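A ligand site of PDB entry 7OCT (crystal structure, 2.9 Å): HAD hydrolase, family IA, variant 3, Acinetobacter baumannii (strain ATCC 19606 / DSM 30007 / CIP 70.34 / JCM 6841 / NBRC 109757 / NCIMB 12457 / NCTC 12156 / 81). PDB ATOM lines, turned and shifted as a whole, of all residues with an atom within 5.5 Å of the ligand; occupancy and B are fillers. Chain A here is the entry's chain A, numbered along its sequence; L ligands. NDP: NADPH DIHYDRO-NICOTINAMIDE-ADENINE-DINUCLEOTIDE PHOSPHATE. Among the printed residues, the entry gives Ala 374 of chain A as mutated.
O1N of the ligand sits at hydrogen-bond distance from N of Ile 255 (3.3 Å). The backbone NH (N) of Ala 254 is in hydrogen-bond range of an oxygen (O1N) of the ligand. The side-chain amino group (NZ) of Lys 420 lies within salt-bridge range of an oxygen (O1X) of the ligand (3.1 Å). The side-chain hydroxyl of Thr 280 lies within hydrogen-bond range of an oxygen (O1X) of the ligand (2.7 Å). The backbone carbonyl oxygen of Leu 336 is in hydrogen-bond range of an oxygen (O3D) of the ligand, at 3.4 Å. N of Arg 281 is in hydrogen-bond range of O2X of the ligand. O7N of the ligand sits at hydrogen-bond distance from N of Val 418 (3.5 Å). N of Asn 282 sits at hydrogen-bond distance from O2X of the ligand (3.5 Å). The backbone NH (N) of Phe 252 lies within hydrogen-bond range of an oxygen (O3B) of the ligand, at 3.3 Å. O of Val 418 lies within hydrogen-bond range of N7N of the ligand, at 3.1 Å. NE of Arg 281 lies within salt-bridge range of O2X of the ligand (3.3 Å).
The side-chain hydroxyl of Ser 279 is in hydrogen-bond range of the backbone NH of Gly 251 (3.0 Å). The backbone NH of Asn 282 is in hydrogen-bond range of the side-chain hydroxyl of Thr 280 (3.3 Å). The backbone NH of Phe 252 sits at hydrogen-bond distance from the backbone carbonyl oxygen of Ser 279. The backbone carbonyl oxygen (O) of Val 414 lies within hydrogen-bond range of the side-chain amino group (NZ) of Lys 527 (2.7 Å).
Merely in contact with the ligand: Gly 251 (3.2 Å), Gly 253 (3.3 Å), Ser 279 (3.8 Å), Cys 335 (3.5 Å), Pro 337 (3.5 Å), Ala 340 (3.5 Å), Glu 344 (3.9 Å), Ile 372 (3.8 Å), Leu 373 (3.3 Å), Ala 374 (3.1 Å), Val 414 (3.7 Å), Arg 416 (3.6 Å) and Met 417 (3.5 Å). Hydrophobic or aromatic side chains within 4 Å of the ligand: Ala 254, Ile 255, Leu 336, Pro 337, Ala 340, Leu 373, Ala 374, Val 414 and Met 417. Of the 30 residues printed, 22 come within 4 Å of the ligand.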
ATOM      1  N   GLY A 251      -2.843 -34.505 -25.986  1.00  0.00           N
ATOM      2  CA  GLY A 251      -3.936 -33.528 -25.824  1.00  0.00           C
ATOM      3  C   GLY A 251      -3.554 -32.171 -26.396  1.00  0.00           C
ATOM      4  O   GLY A 251      -3.228 -31.273 -25.598  1.00  0.00           O
ATOM      5  N   PHE A 252      -3.606 -32.034 -27.722  1.00  0.00           N
ATOM      6  CA  PHE A 252      -3.299 -30.794 -28.471  1.00  0.00           C
ATOM      7  C   PHE A 252      -4.417 -29.773 -28.222  1.00  0.00           C
ATOM      8  O   PHE A 252      -5.163 -29.432 -29.160  1.00  0.00           O
ATOM      9  CB  PHE A 252      -3.109 -31.100 -29.960  1.00  0.00           C
ATOM     10  CG  PHE A 252      -2.607 -29.955 -30.806  1.00  0.00           C
ATOM     11  CD1 PHE A 252      -1.364 -29.395 -30.557  1.00  0.00           C
ATOM     12  CD2 PHE A 252      -3.366 -29.444 -31.844  1.00  0.00           C
ATOM     13  CE1 PHE A 252      -0.896 -28.337 -31.325  1.00  0.00           C
ATOM     14  CE2 PHE A 252      -2.896 -28.399 -32.617  1.00  0.00           C
ATOM     15  CZ  PHE A 252      -1.666 -27.845 -32.359  1.00  0.00           C
ATOM     16  N   GLY A 253      -4.514 -29.305 -26.977  1.00  0.00           N
ATOM     17  CA  GLY A 253      -5.517 -28.320 -26.515  1.00  0.00           C
ATOM     18  C   GLY A 253      -4.897 -26.951 -26.327  1.00  0.00           C
ATOM     19  O   GLY A 253      -3.795 -26.727 -26.856  1.00  0.00           O
ATOM     20  N   ALA A 254      -5.574 -26.074 -25.589  1.00  0.00           N
ATOM     21  CA  ALA A 254      -5.141 -24.691 -25.294  1.00  0.00           C
ATOM     22  C   ALA A 254      -3.715 -24.719 -24.719  1.00  0.00           C
ATOM     23  O   ALA A 254      -2.807 -24.163 -25.361  1.00  0.00           O
ATOM     24  CB  ALA A 254      -6.102 -24.029 -24.336  1.00  0.00           C
ATOM     25  N   ILE A 255      -3.531 -25.375 -23.571  1.00  0.00           N
ATOM     26  CA  ILE A 255      -2.257 -25.381 -22.793  1.00  0.00           C
ATOM     27  C   ILE A 255      -1.217 -26.230 -23.526  1.00  0.00           C
ATOM     28  O   ILE A 255      -0.030 -25.842 -23.518  1.00  0.00           O
ATOM     29  CB  ILE A 255      -2.492 -25.838 -21.343  1.00  0.00           C
ATOM     30  CG1 ILE A 255      -1.412 -25.306 -20.390  1.00  0.00           C
ATOM     31  CG2 ILE A 255      -2.632 -27.352 -21.250  1.00  0.00           C
ATOM     32  CD1 ILE A 255      -1.485 -23.824 -20.145  1.00  0.00           C
ATOM     33  N   GLY A 256      -1.635 -27.335 -24.153  1.00  0.00           N
ATOM     34  CA  GLY A 256      -0.765 -28.248 -24.911  1.00  0.00           C
ATOM     35  C   GLY A 256      -0.079 -27.551 -26.078  1.00  0.00           C
ATOM     36  O   GLY A 256       1.161 -27.602 -26.156  1.00  0.00           O
ATOM     37  N   SER A 279      -1.721 -35.028 -30.121  1.00  0.00           N
ATOM     38  CA  SER A 279      -2.976 -35.809 -30.335  1.00  0.00           C
ATOM     39  C   SER A 279      -4.201 -34.906 -30.183  1.00  0.00           C
ATOM     40  O   SER A 279      -4.217 -34.075 -29.248  1.00  0.00           O
ATOM     41  CB  SER A 279      -3.043 -36.983 -29.409  1.00  0.00           C
ATOM     42  OG  SER A 279      -3.211 -36.569 -28.064  1.00  0.00           O
ATOM     43  N   THR A 280      -5.196 -35.061 -31.064  1.00  0.00           N
ATOM     44  CA  THR A 280      -6.502 -34.340 -31.034  1.00  0.00           C
ATOM     45  C   THR A 280      -7.549 -35.137 -31.822  1.00  0.00           C
ATOM     46  O   THR A 280      -7.158 -35.828 -32.790  1.00  0.00           O
ATOM     47  CB  THR A 280      -6.357 -32.916 -31.577  1.00  0.00           C
ATOM     48  OG1 THR A 280      -7.600 -32.237 -31.370  1.00  0.00           O
ATOM     49  CG2 THR A 280      -6.003 -32.873 -33.050  1.00  0.00           C
ATOM     50  N   ARG A 281      -8.817 -35.029 -31.431  1.00  0.00           N
ATOM     51  CA  ARG A 281      -9.972 -35.647 -32.130  1.00  0.00           C
ATOM     52  C   ARG A 281     -10.490 -34.671 -33.195  1.00  0.00           C
ATOM     53  O   ARG A 281     -11.233 -35.123 -34.091  1.00  0.00           O
ATOM     54  CB  ARG A 281     -11.077 -35.994 -31.125  1.00  0.00           C
ATOM     55  CG  ARG A 281     -10.616 -36.878 -29.967  1.00  0.00           C
ATOM     56  CD  ARG A 281     -11.603 -36.914 -28.823  1.00  0.00           C
ATOM     57  NE  ARG A 281     -11.751 -35.616 -28.178  1.00  0.00           N
ATOM     58  CZ  ARG A 281     -12.633 -35.331 -27.211  1.00  0.00           C
ATOM     59  NH1 ARG A 281     -13.472 -36.252 -26.778  1.00  0.00           N
ATOM     60  NH2 ARG A 281     -12.679 -34.112 -26.706  1.00  0.00           N
ATOM     61  N   ASN A 282     -10.115 -33.393 -33.099  1.00  0.00           N
ATOM     62  CA  ASN A 282     -10.528 -32.296 -34.024  1.00  0.00           C
ATOM     63  C   ASN A 282      -9.825 -32.482 -35.377  1.00  0.00           C
ATOM     64  O   ASN A 282      -8.598 -32.291 -35.438  1.00  0.00           O
ATOM     65  CB  ASN A 282     -10.236 -30.921 -33.424  1.00  0.00           C
ATOM     66  CG  ASN A 282     -10.938 -29.785 -34.137  1.00  0.00           C
ATOM     67  OD1 ASN A 282     -11.173 -29.843 -35.343  1.00  0.00           O
ATOM     68  ND2 ASN A 282     -11.269 -28.736 -33.407  1.00  0.00           N
ATOM     69  N   CYS A 335      -1.797 -33.197 -21.376  1.00  0.00           N
ATOM     70  CA  CYS A 335      -2.514 -31.891 -21.317  1.00  0.00           C
ATOM     71  C   CYS A 335      -4.012 -32.118 -21.508  1.00  0.00           C
ATOM     72  O   CYS A 335      -4.612 -31.457 -22.369  1.00  0.00           O
ATOM     73  CB  CYS A 335      -1.961 -30.944 -22.383  1.00  0.00           C
ATOM     74  SG  CYS A 335      -0.162 -30.786 -22.334  1.00  0.00           S
ATOM     75  N   LEU A 336      -4.595 -33.022 -20.698  1.00  0.00           N
ATOM     76  CA  LEU A 336      -6.043 -33.360 -20.702  1.00  0.00           C
ATOM     77  C   LEU A 336      -6.720 -32.709 -19.503  1.00  0.00           C
ATOM     78  O   LEU A 336      -6.057 -32.387 -18.515  1.00  0.00           O
ATOM     79  CB  LEU A 336      -6.194 -34.885 -20.642  1.00  0.00           C
ATOM     80  CG  LEU A 336      -5.487 -35.683 -21.733  1.00  0.00           C
ATOM     81  CD1 LEU A 336      -5.617 -37.169 -21.460  1.00  0.00           C
ATOM     82  CD2 LEU A 336      -6.046 -35.339 -23.104  1.00  0.00           C
ATOM     83  N   PRO A 337      -8.053 -32.504 -19.531  1.00  0.00           N
ATOM     84  CA  PRO A 337      -8.815 -32.153 -18.334  1.00  0.00           C
ATOM     85  C   PRO A 337      -8.968 -33.357 -17.399  1.00  0.00           C
ATOM     86  O   PRO A 337      -8.557 -34.448 -17.760  1.00  0.00           O
ATOM     87  CB  PRO A 337     -10.190 -31.711 -18.861  1.00  0.00           C
ATOM     88  CG  PRO A 337     -10.022 -31.587 -20.373  1.00  0.00           C
ATOM     89  CD  PRO A 337      -8.902 -32.540 -20.735  1.00  0.00           C
ATOM     90  N   GLU A 338      -9.577 -33.147 -16.227  1.00  0.00           N
ATOM     91  CA  GLU A 338      -9.793 -34.178 -15.176  1.00  0.00           C
ATOM     92  C   GLU A 338     -10.812 -35.216 -15.668  1.00  0.00           C
ATOM     93  O   GLU A 338     -10.699 -36.383 -15.257  1.00  0.00           O
ATOM     94  CB  GLU A 338     -10.280 -33.524 -13.880  1.00  0.00           C
ATOM     95  CG  GLU A 338     -10.269 -34.462 -12.677  1.00  0.00           C
ATOM     96  CD  GLU A 338     -10.737 -33.840 -11.374  1.00  0.00           C
ATOM     97  OE1 GLU A 338     -10.516 -34.467 -10.314  1.00  0.00           O
ATOM     98  OE2 GLU A 338     -11.314 -32.740 -11.408  1.00  0.00           O
ATOM     99  N   GLN A 339     -11.757 -34.808 -16.534  1.00  0.00           N
ATOM    100  CA  GLN A 339     -12.881 -35.652 -17.018  1.00  0.00           C
ATOM    101  C   GLN A 339     -12.373 -36.680 -18.037  1.00  0.00           C
ATOM    102  O   GLN A 339     -13.024 -37.735 -18.184  1.00  0.00           O
ATOM    103  CB  GLN A 339     -13.975 -34.785 -17.644  1.00  0.00           C
ATOM    104  CG  GLN A 339     -14.797 -34.000 -16.626  1.00  0.00           C
ATOM    105  CD  GLN A 339     -14.072 -32.786 -16.085  1.00  0.00           C
ATOM    106  OE1 GLN A 339     -13.007 -32.399 -16.552  1.00  0.00           O
ATOM    107  NE2 GLN A 339     -14.665 -32.174 -15.068  1.00  0.00           N
ATOM    108  N   ALA A 340     -11.257 -36.384 -18.721  1.00  0.00           N
ATOM    109  CA  ALA A 340     -10.721 -37.162 -19.869  1.00  0.00           C
ATOM    110  C   ALA A 340      -9.695 -38.205 -19.406  1.00  0.00           C
ATOM    111  O   ALA A 340      -9.229 -38.977 -20.278  1.00  0.00           O
ATOM    112  CB  ALA A 340     -10.114 -36.208 -20.867  1.00  0.00           C
ATOM    113  N   SER A 343     -10.948 -42.111 -19.473  1.00  0.00           N
ATOM    114  CA  SER A 343     -11.145 -42.532 -20.887  1.00  0.00           C
ATOM    115  C   SER A 343      -9.786 -42.766 -21.558  1.00  0.00           C
ATOM    116  O   SER A 343      -9.611 -43.837 -22.181  1.00  0.00           O
ATOM    117  CB  SER A 343     -11.961 -41.515 -21.643  1.00  0.00           C
ATOM    118  OG  SER A 343     -13.250 -41.376 -21.071  1.00  0.00           O
ATOM    119  N   GLU A 344      -8.857 -41.813 -21.436  1.00  0.00           N
ATOM    120  CA  GLU A 344      -7.556 -41.791 -22.153  1.00  0.00           C
ATOM    121  C   GLU A 344      -6.545 -42.700 -21.458  1.00  0.00           C
ATOM    122  O   GLU A 344      -5.544 -43.063 -22.118  1.00  0.00           O
ATOM    123  CB  GLU A 344      -7.028 -40.354 -22.260  1.00  0.00           C
ATOM    124  CG  GLU A 344      -7.867 -39.457 -23.156  1.00  0.00           C
ATOM    125  CD  GLU A 344      -7.816 -39.786 -24.632  1.00  0.00           C
ATOM    126  OE1 GLU A 344      -8.885 -39.887 -25.255  1.00  0.00           O
ATOM    127  OE2 GLU A 344      -6.694 -39.927 -25.163  1.00  0.00           O
ATOM    128  N   ILE A 372       0.100 -32.195 -16.872  1.00  0.00           N
ATOM    129  CA  ILE A 372      -0.454 -30.816 -17.014  1.00  0.00           C
ATOM    130  C   ILE A 372      -1.946 -30.883 -16.644  1.00  0.00           C
ATOM    131  O   ILE A 372      -2.775 -31.078 -17.561  1.00  0.00           O
ATOM    132  CB  ILE A 372      -0.219 -30.251 -18.427  1.00  0.00           C
ATOM    133  CG1 ILE A 372       1.199 -30.511 -18.940  1.00  0.00           C
ATOM    134  CG2 ILE A 372      -0.568 -28.768 -18.483  1.00  0.00           C
ATOM    135  CD1 ILE A 372       2.293 -29.988 -18.035  1.00  0.00           C
ATOM    136  N   LEU A 373      -2.255 -30.741 -15.360  1.00  0.00           N
ATOM    137  CA  LEU A 373      -3.632 -30.843 -14.779  1.00  0.00           C
ATOM    138  C   LEU A 373      -3.720 -29.917 -13.558  1.00  0.00           C
ATOM    139  O   LEU A 373      -2.810 -29.978 -12.710  1.00  0.00           O
ATOM    140  CB  LEU A 373      -3.903 -32.304 -14.412  1.00  0.00           C
ATOM    141  CG  LEU A 373      -5.318 -32.636 -13.955  1.00  0.00           C
ATOM    142  CD1 LEU A 373      -6.329 -32.324 -15.058  1.00  0.00           C
ATOM    143  CD2 LEU A 373      -5.425 -34.098 -13.541  1.00  0.00           C
ATOM    144  N   ALA A 374      -4.775 -29.094 -13.493  1.00  0.00           N
ATOM    145  CA  ALA A 374      -4.906 -27.961 -12.549  1.00  0.00           C
ATOM    146  C   ALA A 374      -5.179 -28.439 -11.113  1.00  0.00           C
ATOM    147  O   ALA A 374      -4.872 -27.675 -10.182  1.00  0.00           O
ATOM    148  CB  ALA A 374      -6.002 -27.021 -13.026  1.00  0.00           C
ATOM    149  N   LYS A 375      -5.734 -29.641 -10.946  1.00  0.00           N
ATOM    150  CA  LYS A 375      -6.200 -30.164  -9.637  1.00  0.00           C
ATOM    151  C   LYS A 375      -4.999 -30.607  -8.795  1.00  0.00           C
ATOM    152  O   LYS A 375      -3.977 -31.023  -9.385  1.00  0.00           O
ATOM    153  CB  LYS A 375      -7.182 -31.327  -9.829  1.00  0.00           C
ATOM    154  CG  LYS A 375      -8.227 -31.146 -10.926  1.00  0.00           C
ATOM    155  CD  LYS A 375      -8.950 -29.802 -10.883  1.00  0.00           C
ATOM    156  CE  LYS A 375      -9.913 -29.611 -12.048  1.00  0.00           C
ATOM    157  NZ  LYS A 375      -9.213 -29.610 -13.350  1.00  0.00           N
ATOM    158  N   VAL A 414       1.292 -24.679 -13.503  1.00  0.00           N
ATOM    159  CA  VAL A 414       1.252 -23.803 -14.713  1.00  0.00           C
ATOM    160  C   VAL A 414       0.552 -22.491 -14.353  1.00  0.00           C
ATOM    161  O   VAL A 414      -0.454 -22.557 -13.612  1.00  0.00           O
ATOM    162  CB  VAL A 414       0.556 -24.523 -15.883  1.00  0.00           C
ATOM    163  CG1 VAL A 414       0.323 -23.589 -17.072  1.00  0.00           C
ATOM    164  CG2 VAL A 414       1.321 -25.762 -16.319  1.00  0.00           C
ATOM    165  N   ASN A 415       1.057 -21.356 -14.852  1.00  0.00           N
ATOM    166  CA  ASN A 415       0.539 -19.996 -14.546  1.00  0.00           C
ATOM    167  C   ASN A 415       0.079 -19.279 -15.818  1.00  0.00           C
ATOM    168  O   ASN A 415      -0.549 -18.209 -15.678  1.00  0.00           O
ATOM    169  CB  ASN A 415       1.594 -19.168 -13.788  1.00  0.00           C
ATOM    170  CG  ASN A 415       1.829 -19.656 -12.379  1.00  0.00           C
ATOM    171  OD1 ASN A 415       0.873 -19.896 -11.636  1.00  0.00           O
ATOM    172  ND2 ASN A 415       3.081 -19.805 -11.996  1.00  0.00           N
ATOM    173  N   ARG A 416       0.348 -19.820 -17.009  1.00  0.00           N
ATOM    174  CA  ARG A 416      -0.034 -19.193 -18.303  1.00  0.00           C
ATOM    175  C   ARG A 416      -1.477 -19.562 -18.646  1.00  0.00           C
ATOM    176  O   ARG A 416      -1.754 -20.765 -18.831  1.00  0.00           O
ATOM    177  CB  ARG A 416       0.897 -19.637 -19.439  1.00  0.00           C
ATOM    178  CG  ARG A 416       0.532 -19.042 -20.793  1.00  0.00           C
ATOM    179  CD  ARG A 416       1.421 -19.514 -21.931  1.00  0.00           C
ATOM    180  NE  ARG A 416       2.715 -18.852 -21.927  1.00  0.00           N
ATOM    181  CZ  ARG A 416       3.614 -18.922 -22.913  1.00  0.00           C
ATOM    182  NH1 ARG A 416       3.365 -19.621 -24.007  1.00  0.00           N
ATOM    183  NH2 ARG A 416       4.763 -18.272 -22.803  1.00  0.00           N
ATOM    184  N   MET A 417      -2.357 -18.561 -18.752  1.00  0.00           N
ATOM    185  CA  MET A 417      -3.753 -18.704 -19.255  1.00  0.00           C
ATOM    186  C   MET A 417      -3.727 -18.708 -20.782  1.00  0.00           C
ATOM    187  O   MET A 417      -3.117 -17.781 -21.361  1.00  0.00           O
ATOM    188  CB  MET A 417      -4.647 -17.552 -18.770  1.00  0.00           C
ATOM    189  CG  MET A 417      -4.696 -17.383 -17.267  1.00  0.00           C
ATOM    190  SD  MET A 417      -5.495 -18.767 -16.406  1.00  0.00           S
ATOM    191  CE  MET A 417      -4.069 -19.739 -15.922  1.00  0.00           C
ATOM    192  N   VAL A 418      -4.342 -19.719 -21.412  1.00  0.00           N
ATOM    193  CA  VAL A 418      -4.411 -19.871 -22.900  1.00  0.00           C
ATOM    194  C   VAL A 418      -5.860 -20.194 -23.296  1.00  0.00           C
ATOM    195  O   VAL A 418      -6.550 -20.873 -22.512  1.00  0.00           O
ATOM    196  CB  VAL A 418      -3.449 -20.951 -23.404  1.00  0.00           C
ATOM    197  CG1 VAL A 418      -3.416 -21.006 -24.921  1.00  0.00           C
ATOM    198  CG2 VAL A 418      -2.039 -20.779 -22.841  1.00  0.00           C
ATOM    199  N   SER A 419      -6.276 -19.725 -24.474  1.00  0.00           N
ATOM    200  CA  SER A 419      -7.595 -20.004 -25.103  1.00  0.00           C
ATOM    201  C   SER A 419      -7.372 -20.599 -26.497  1.00  0.00           C
ATOM    202  O   SER A 419      -6.646 -19.984 -27.302  1.00  0.00           O
ATOM    203  CB  SER A 419      -8.433 -18.758 -25.167  1.00  0.00           C
ATOM    204  OG  SER A 419      -7.774 -17.733 -25.878  1.00  0.00           O
ATOM    205  N   LYS A 420      -7.977 -21.765 -26.767  1.00  0.00           N
ATOM    206  CA  LYS A 420      -7.953 -22.452 -28.085  1.00  0.00           C
ATOM    207  C   LYS A 420      -8.949 -21.753 -29.018  1.00  0.00           C
ATOM    208  O   LYS A 420     -10.051 -21.402 -28.549  1.00  0.00           O
ATOM    209  CB  LYS A 420      -8.279 -23.935 -27.925  1.00  0.00           C
ATOM    210  CG  LYS A 420      -8.119 -24.783 -29.177  1.00  0.00           C
ATOM    211  CD  LYS A 420      -8.510 -26.233 -28.971  1.00  0.00           C
ATOM    212  CE  LYS A 420      -8.283 -27.082 -30.203  1.00  0.00           C
ATOM    213  NZ  LYS A 420      -8.545 -28.526 -29.939  1.00  0.00           N
ATOM    214  N   LYS A 527       0.073 -21.135  -5.879  1.00  0.00           N
ATOM    215  CA  LYS A 527      -0.903 -21.215  -7.003  1.00  0.00           C
ATOM    216  C   LYS A 527      -2.334 -21.226  -6.449  1.00  0.00           C
ATOM    217  O   LYS A 527      -3.218 -20.609  -7.087  1.00  0.00           O
ATOM    218  CB  LYS A 527      -0.638 -22.484  -7.836  1.00  0.00           C
ATOM    219  CG  LYS A 527      -1.622 -22.738  -8.974  1.00  0.00           C
ATOM    220  CD  LYS A 527      -1.607 -21.662 -10.045  1.00  0.00           C
ATOM    221  CE  LYS A 527      -2.575 -21.945 -11.168  1.00  0.00           C
ATOM    222  NZ  LYS A 527      -2.339 -21.037 -12.322  1.00  0.00           N
HETATM  223  PA  NDP L   1      -8.772 -28.352 -23.759  1.00  0.00           P
HETATM  224  O1A NDP L   1     -10.183 -28.797 -23.535  1.00  0.00           O
HETATM  225  O2A NDP L   1      -8.479 -26.991 -24.314  1.00  0.00           O
HETATM  226  O5B NDP L   1      -8.021 -29.492 -24.688  1.00  0.00           O
HETATM  227  C5B NDP L   1      -7.736 -30.554 -23.824  1.00  0.00           C
HETATM  228  C4B NDP L   1      -7.287 -31.783 -24.608  1.00  0.00           C
HETATM  229  O4B NDP L   1      -7.930 -32.919 -24.027  1.00  0.00           O
HETATM  230  C3B NDP L   1      -7.672 -31.707 -26.117  1.00  0.00           C
HETATM  231  O3B NDP L   1      -6.780 -32.462 -26.873  1.00  0.00           O
HETATM  232  C2B NDP L   1      -9.047 -32.384 -26.128  1.00  0.00           C
HETATM  233  O2B NDP L   1      -9.318 -33.048 -27.252  1.00  0.00           O
HETATM  234  C1B NDP L   1      -8.880 -33.426 -24.963  1.00  0.00           C
HETATM  235  N9A NDP L   1     -10.154 -33.628 -24.237  1.00  0.00           N
HETATM  236  C8A NDP L   1     -10.958 -32.677 -23.596  1.00  0.00           C
HETATM  237  N7A NDP L   1     -12.064 -33.194 -23.025  1.00  0.00           N
HETATM  238  C5A NDP L   1     -11.974 -34.570 -23.326  1.00  0.00           C
HETATM  239  C6A NDP L   1     -12.821 -35.649 -23.014  1.00  0.00           C
HETATM  240  N6A NDP L   1     -13.976 -35.451 -22.292  1.00  0.00           N
HETATM  241  N1A NDP L   1     -12.514 -36.944 -23.416  1.00  0.00           N
HETATM  242  C2A NDP L   1     -11.338 -37.070 -24.136  1.00  0.00           C
HETATM  243  N3A NDP L   1     -10.432 -36.135 -24.511  1.00  0.00           N
HETATM  244  C4A NDP L   1     -10.779 -34.858 -24.080  1.00  0.00           C
HETATM  245  O3  NDP L   1      -8.215 -28.408 -22.197  1.00  0.00           O
HETATM  246  PN  NDP L   1      -7.141 -27.251 -21.965  1.00  0.00           P
HETATM  247  O1N NDP L   1      -5.939 -27.528 -22.777  1.00  0.00           O
HETATM  248  O2N NDP L   1      -7.753 -25.869 -21.838  1.00  0.00           O
HETATM  249  O5D NDP L   1      -6.488 -27.433 -20.340  1.00  0.00           O
HETATM  250  C5D NDP L   1      -6.113 -28.746 -20.152  1.00  0.00           C
HETATM  251  C4D NDP L   1      -5.646 -28.898 -18.712  1.00  0.00           C
HETATM  252  O4D NDP L   1      -4.663 -27.891 -18.418  1.00  0.00           O
HETATM  253  C3D NDP L   1      -6.864 -28.650 -17.773  1.00  0.00           C
HETATM  254  O3D NDP L   1      -6.797 -29.564 -16.729  1.00  0.00           O
HETATM  255  C2D NDP L   1      -6.613 -27.223 -17.282  1.00  0.00           C
HETATM  256  O2D NDP L   1      -7.062 -27.006 -15.978  1.00  0.00           O
HETATM  257  C1D NDP L   1      -5.060 -27.175 -17.285  1.00  0.00           C
HETATM  258  N1N NDP L   1      -4.559 -25.782 -17.405  1.00  0.00           N
HETATM  259  C2N NDP L   1      -5.045 -24.948 -18.407  1.00  0.00           C
HETATM  260  C3N NDP L   1      -4.763 -23.609 -18.383  1.00  0.00           C
HETATM  261  C7N NDP L   1      -5.478 -22.760 -19.347  1.00  0.00           C
HETATM  262  O7N NDP L   1      -5.996 -21.679 -19.047  1.00  0.00           O
HETATM  263  N7N NDP L   1      -5.555 -23.174 -20.673  1.00  0.00           N
HETATM  264  C4N NDP L   1      -4.064 -23.000 -17.226  1.00  0.00           C
HETATM  265  C5N NDP L   1      -3.281 -24.000 -16.463  1.00  0.00           C
HETATM  266  C6N NDP L   1      -3.563 -25.308 -16.521  1.00  0.00           C
HETATM  267  P2B NDP L   1      -9.797 -31.985 -28.669  1.00  0.00           P
HETATM  268  O1X NDP L   1      -8.436 -31.456 -28.972  1.00  0.00           O
HETATM  269  O2X NDP L   1     -10.403 -32.990 -29.652  1.00  0.00           O
HETATM  270  O3X NDP L   1     -10.760 -31.065 -27.951  1.00  0.00           O
